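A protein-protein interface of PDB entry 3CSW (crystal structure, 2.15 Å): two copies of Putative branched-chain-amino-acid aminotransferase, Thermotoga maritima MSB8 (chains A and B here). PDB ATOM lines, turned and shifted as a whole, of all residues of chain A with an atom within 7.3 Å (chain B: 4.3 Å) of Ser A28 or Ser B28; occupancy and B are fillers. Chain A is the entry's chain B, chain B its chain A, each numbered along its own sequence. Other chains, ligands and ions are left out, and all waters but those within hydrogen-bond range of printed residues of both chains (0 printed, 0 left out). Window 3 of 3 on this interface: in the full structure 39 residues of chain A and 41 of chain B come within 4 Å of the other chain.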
ATOM      1  N   TRP A  17     -22.273  -9.034 -37.906  1.00  0.00           N
ATOM      2  CA  TRP A  17     -21.278  -8.818 -36.864  1.00  0.00           C
ATOM      3  C   TRP A  17     -19.978  -9.418 -37.355  1.00  0.00           C
ATOM      4  O   TRP A  17     -19.968 -10.539 -37.859  1.00  0.00           O
ATOM      5  CB  TRP A  17     -21.758  -9.493 -35.575  1.00  0.00           C
ATOM      6  CG  TRP A  17     -20.783  -9.534 -34.414  1.00  0.00           C
ATOM      7  CD1 TRP A  17     -20.158 -10.642 -33.908  1.00  0.00           C
ATOM      8  CD2 TRP A  17     -20.352  -8.431 -33.606  1.00  0.00           C
ATOM      9  NE1 TRP A  17     -19.364 -10.293 -32.847  1.00  0.00           N
ATOM     10  CE2 TRP A  17     -19.462  -8.943 -32.642  1.00  0.00           C
ATOM     11  CE3 TRP A  17     -20.625  -7.059 -33.612  1.00  0.00           C
ATOM     12  CZ2 TRP A  17     -18.846  -8.135 -31.688  1.00  0.00           C
ATOM     13  CZ3 TRP A  17     -20.012  -6.252 -32.657  1.00  0.00           C
ATOM     14  CH2 TRP A  17     -19.136  -6.796 -31.709  1.00  0.00           C
ATOM     15  N   ARG A  18     -18.903  -8.646 -37.269  1.00  0.00           N
ATOM     16  CA  ARG A  18     -17.573  -9.105 -37.666  1.00  0.00           C
ATOM     17  C   ARG A  18     -17.524  -9.790 -39.037  1.00  0.00           C
ATOM     18  O   ARG A  18     -17.161 -10.957 -39.148  1.00  0.00           O
ATOM     19  CB  ARG A  18     -17.002 -10.025 -36.591  1.00  0.00           C
ATOM     20  CG  ARG A  18     -16.566  -9.284 -35.371  1.00  0.00           C
ATOM     21  CD  ARG A  18     -16.172 -10.232 -34.289  1.00  0.00           C
ATOM     22  NE  ARG A  18     -15.275  -9.588 -33.334  1.00  0.00           N
ATOM     23  CZ  ARG A  18     -13.943  -9.664 -33.363  1.00  0.00           C
ATOM     24  NH1 ARG A  18     -13.302 -10.371 -34.305  1.00  0.00           N
ATOM     25  NH2 ARG A  18     -13.240  -9.026 -32.425  1.00  0.00           N
ATOM     26  N   GLU A  26     -27.464 -17.322 -30.152  1.00  0.00           N
ATOM     27  CA  GLU A  26     -26.460 -17.068 -29.122  1.00  0.00           C
ATOM     28  C   GLU A  26     -25.284 -16.378 -29.784  1.00  0.00           C
ATOM     29  O   GLU A  26     -25.158 -16.403 -31.001  1.00  0.00           O
ATOM     30  CB  GLU A  26     -26.014 -18.346 -28.387  1.00  0.00           C
ATOM     31  CG  GLU A  26     -27.006 -18.804 -27.288  1.00  0.00           C
ATOM     32  CD  GLU A  26     -26.336 -19.321 -26.004  1.00  0.00           C
ATOM     33  OE1 GLU A  26     -25.091 -19.430 -25.945  1.00  0.00           O
ATOM     34  OE2 GLU A  26     -27.074 -19.610 -25.037  1.00  0.00           O
ATOM     35  N   ILE A  27     -24.452 -15.732 -28.979  1.00  0.00           N
ATOM     36  CA  ILE A  27     -23.293 -15.014 -29.480  1.00  0.00           C
ATOM     37  C   ILE A  27     -22.111 -15.299 -28.553  1.00  0.00           C
ATOM     38  O   ILE A  27     -22.270 -15.316 -27.328  1.00  0.00           O
ATOM     39  CB  ILE A  27     -23.591 -13.480 -29.590  1.00  0.00           C
ATOM     40  CG1 ILE A  27     -22.528 -12.763 -30.432  1.00  0.00           C
ATOM     41  CG2 ILE A  27     -23.733 -12.822 -28.200  1.00  0.00           C
ATOM     42  CD1 ILE A  27     -22.845 -11.290 -30.716  1.00  0.00           C
ATOM     43  N   SER A  28     -20.949 -15.584 -29.132  1.00  0.00           N
ATOM     44  CA  SER A  28     -19.719 -15.687 -28.348  1.00  0.00           C
ATOM     45  C   SER A  28     -18.917 -14.424 -28.588  1.00  0.00           C
ATOM     46  O   SER A  28     -18.750 -13.992 -29.730  1.00  0.00           O
ATOM     47  CB  SER A  28     -18.901 -16.924 -28.705  1.00  0.00           C
ATOM     48  OG  SER A  28     -19.496 -18.075 -28.147  1.00  0.00           O
ATOM     49  N   LEU A  29     -18.446 -13.821 -27.504  1.00  0.00           N
ATOM     50  CA  LEU A  29     -17.724 -12.563 -27.584  1.00  0.00           C
ATOM     51  C   LEU A  29     -16.434 -12.672 -26.841  1.00  0.00           C
ATOM     52  O   LEU A  29     -16.334 -13.425 -25.870  1.00  0.00           O
ATOM     53  CB  LEU A  29     -18.513 -11.432 -26.908  1.00  0.00           C
ATOM     54  CG  LEU A  29     -19.863 -11.028 -27.465  1.00  0.00           C
ATOM     55  CD1 LEU A  29     -20.582 -10.173 -26.438  1.00  0.00           C
ATOM     56  CD2 LEU A  29     -19.668 -10.292 -28.780  1.00  0.00           C
ATOM     57  N   ASP A  30     -15.461 -11.881 -27.277  1.00  0.00           N
ATOM     58  CA  ASP A  30     -14.267 -11.676 -26.488  1.00  0.00           C
ATOM     59  C   ASP A  30     -14.798 -11.148 -25.164  1.00  0.00           C
ATOM     60  O   ASP A  30     -15.632 -10.244 -25.160  1.00  0.00           O
ATOM     61  CB  ASP A  30     -13.344 -10.652 -27.145  1.00  0.00           C
ATOM     62  CG  ASP A  30     -12.203 -10.238 -26.241  1.00  0.00           C
ATOM     63  OD1 ASP A  30     -11.684 -11.100 -25.489  1.00  0.00           O
ATOM     64  OD2 ASP A  30     -11.831  -9.042 -26.279  1.00  0.00           O
ATOM     65  N   PHE A  31     -14.356 -11.719 -24.051  1.00  0.00           N
ATOM     66  CA  PHE A  31     -14.935 -11.346 -22.769  1.00  0.00           C
ATOM     67  C   PHE A  31     -14.711  -9.882 -22.415  1.00  0.00           C
ATOM     68  O   PHE A  31     -15.618  -9.220 -21.931  1.00  0.00           O
ATOM     69  CB  PHE A  31     -14.430 -12.210 -21.623  1.00  0.00           C
ATOM     70  CG  PHE A  31     -14.971 -11.781 -20.302  1.00  0.00           C
ATOM     71  CD1 PHE A  31     -16.276 -12.081 -19.953  1.00  0.00           C
ATOM     72  CD2 PHE A  31     -14.212 -11.013 -19.443  1.00  0.00           C
ATOM     73  CE1 PHE A  31     -16.801 -11.646 -18.751  1.00  0.00           C
ATOM     74  CE2 PHE A  31     -14.724 -10.592 -18.248  1.00  0.00           C
ATOM     75  CZ  PHE A  31     -16.020 -10.904 -17.901  1.00  0.00           C
ATOM     76  N   TRP B  17     -20.500 -17.661 -14.138  1.00  0.00           N
ATOM     77  CA  TRP B  17     -21.528 -17.323 -15.107  1.00  0.00           C
ATOM     78  C   TRP B  17     -22.391 -18.555 -15.349  1.00  0.00           C
ATOM     79  O   TRP B  17     -21.872 -19.640 -15.590  1.00  0.00           O
ATOM     80  CB  TRP B  17     -20.845 -16.848 -16.397  1.00  0.00           C
ATOM     81  CG  TRP B  17     -21.748 -16.442 -17.532  1.00  0.00           C
ATOM     82  CD1 TRP B  17     -21.709 -16.913 -18.816  1.00  0.00           C
ATOM     83  CD2 TRP B  17     -22.805 -15.475 -17.494  1.00  0.00           C
ATOM     84  NE1 TRP B  17     -22.674 -16.303 -19.571  1.00  0.00           N
ATOM     85  CE2 TRP B  17     -23.358 -15.412 -18.788  1.00  0.00           C
ATOM     86  CE3 TRP B  17     -23.336 -14.653 -16.493  1.00  0.00           C
ATOM     87  CZ2 TRP B  17     -24.418 -14.560 -19.108  1.00  0.00           C
ATOM     88  CZ3 TRP B  17     -24.394 -13.806 -16.815  1.00  0.00           C
ATOM     89  CH2 TRP B  17     -24.920 -13.769 -18.108  1.00  0.00           C
ATOM     90  N   ARG B  18     -23.704 -18.379 -15.237  1.00  0.00           N
ATOM     91  CA  ARG B  18     -24.668 -19.448 -15.466  1.00  0.00           C
ATOM     92  C   ARG B  18     -24.294 -20.733 -14.714  1.00  0.00           C
ATOM     93  O   ARG B  18     -24.126 -21.801 -15.311  1.00  0.00           O
ATOM     94  CB  ARG B  18     -24.836 -19.698 -16.976  1.00  0.00           C
ATOM     95  CG  ARG B  18     -25.087 -18.412 -17.786  1.00  0.00           C
ATOM     96  CD  ARG B  18     -25.821 -18.631 -19.131  1.00  0.00           C
ATOM     97  NE  ARG B  18     -25.131 -19.553 -20.045  1.00  0.00           N
ATOM     98  CZ  ARG B  18     -25.286 -19.583 -21.373  1.00  0.00           C
ATOM     99  NH1 ARG B  18     -26.099 -18.730 -22.000  1.00  0.00           N
ATOM    100  NH2 ARG B  18     -24.602 -20.469 -22.090  1.00  0.00           N
ATOM    101  N   ILE B  27     -16.973 -15.452 -23.725  1.00  0.00           N
ATOM    102  CA  ILE B  27     -18.247 -15.562 -23.014  1.00  0.00           C
ATOM    103  C   ILE B  27     -19.335 -15.886 -24.035  1.00  0.00           C
ATOM    104  O   ILE B  27     -19.368 -15.303 -25.118  1.00  0.00           O
ATOM    105  CB  ILE B  27     -18.581 -14.287 -22.175  1.00  0.00           C
ATOM    106  CG1 ILE B  27     -19.687 -14.576 -21.146  1.00  0.00           C
ATOM    107  CG2 ILE B  27     -18.936 -13.104 -23.081  1.00  0.00           C
ATOM    108  CD1 ILE B  27     -19.942 -13.433 -20.181  1.00  0.00           C
ATOM    109  N   SER B  28     -20.180 -16.860 -23.694  1.00  0.00           N
ATOM    110  CA  SER B  28     -21.315 -17.260 -24.524  1.00  0.00           C
ATOM    111  C   SER B  28     -22.596 -16.829 -23.854  1.00  0.00           C
ATOM    112  O   SER B  28     -22.928 -17.301 -22.763  1.00  0.00           O
ATOM    113  CB  SER B  28     -21.354 -18.773 -24.726  1.00  0.00           C
ATOM    114  OG  SER B  28     -20.477 -19.154 -25.758  1.00  0.00           O
ATOM    115  N   LEU B  29     -23.322 -15.937 -24.512  1.00  0.00           N
ATOM    116  CA  LEU B  29     -24.586 -15.472 -23.970  1.00  0.00           C
ATOM    117  C   LEU B  29     -25.640 -15.360 -25.061  1.00  0.00           C
ATOM    118  O   LEU B  29     -25.317 -15.277 -26.241  1.00  0.00           O
ATOM    119  CB  LEU B  29     -24.396 -14.151 -23.210  1.00  0.00           C
ATOM    120  CG  LEU B  29     -23.944 -12.879 -23.929  1.00  0.00           C
ATOM    121  CD1 LEU B  29     -23.982 -11.744 -22.927  1.00  0.00           C
ATOM    122  CD2 LEU B  29     -22.566 -13.007 -24.534  1.00  0.00           C
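OG of Ser B28 sits at hydrogen-bond distance from OG of Ser A28 (2.8 Å). OE2 of Glu A26 is in salt-bridge range of NH1 of Arg B18, at 3.3 Å. The backbone carbonyl oxygen (O) of Ile B27 is in hydrogen-bond range of the backbone NH (N) of Leu A29 (3.0 Å). N of Ile A27 is in hydrogen-bond range of O of Leu B29.
The backbone carbonyl oxygen of Ser B28 is in hydrogen-bond range of the indole nitrogen of Trp B17.
Glu A26 touches Ser B28. CA of Glu A26 touches O of Leu B29 (3.6 Å). Ile A27 touches Ile B27. Ser B28 touches Ile A27. Ile B27 touches Ser A28. Leu A29 touches Leu B29 (CD1 to CD2, 3.9 Å). Phe A31 touches Ile B27.
Of chain B, only Ile B27 and Ser B28 come within 4 Å of Ser A28. Of the printed residues of chain A, Ser B28 touches Glu A26 (3.99 Å), Ile A27 (3.5 Å) and Ser A28 (2.8 Å). Of the printed residues of chain A, Arg B18 touches Glu A26. Printed residues of chain B within 4 Å of Phe A31: Ile B27 (3.9 Å). Of the printed residues of chain B, Glu A26 touches Arg B18 (3.3 Å), Ser B28 (3.99 Å) and Leu B29 (3.6 Å). Printed residues of chain A within 4 Å of Ile B27: Ile A27, Ser A28, Leu A29 and Phe A31. Arg A18 touches none of the printed residues of chain B. Asp A30 touches none of the printed residues of chain B. The nearest printed residue of chain B that does not touch Phe A31 is Trp B17 (7.0 Å).
Printed residues of chain B that touch a printed residue of chain A: Arg B18, Ile B27, Ser B28 and Leu B29. Hydrophobic or aromatic side chains of chain B that line the printed part of chain A: Ile B27 and Leu B29. Of the 8 printed residues of chain A, 5 touch a printed residue of chain B. Hydrophobic or aromatic side chains of chain A within 4 Å of the printed part of chain B: Ile A27, Leu A29 and Phe A31. Among the printed residues, 11 pairs touch across the chains. Among the printed residues, Asp or Glu carboxylates within 4 Å of a Lys or Arg side-chain nitrogen of the other chain: Glu A26 with Arg B18 (3.3 Å).
Ile A27 touches its own counterpart, Ile B27. Ile A27 touches Ser B28, and with the chains exchanged Ser A28 touches Ile B27. Ile A27 touches Leu B29, and with the chains exchanged Leu A29 touches Ile B27. Ser A28 touches its own counterpart, Ser B28. Of the 11 pairs that touch across the chains among the printed residues, 7 have their exchanged pair printed and touching as well.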
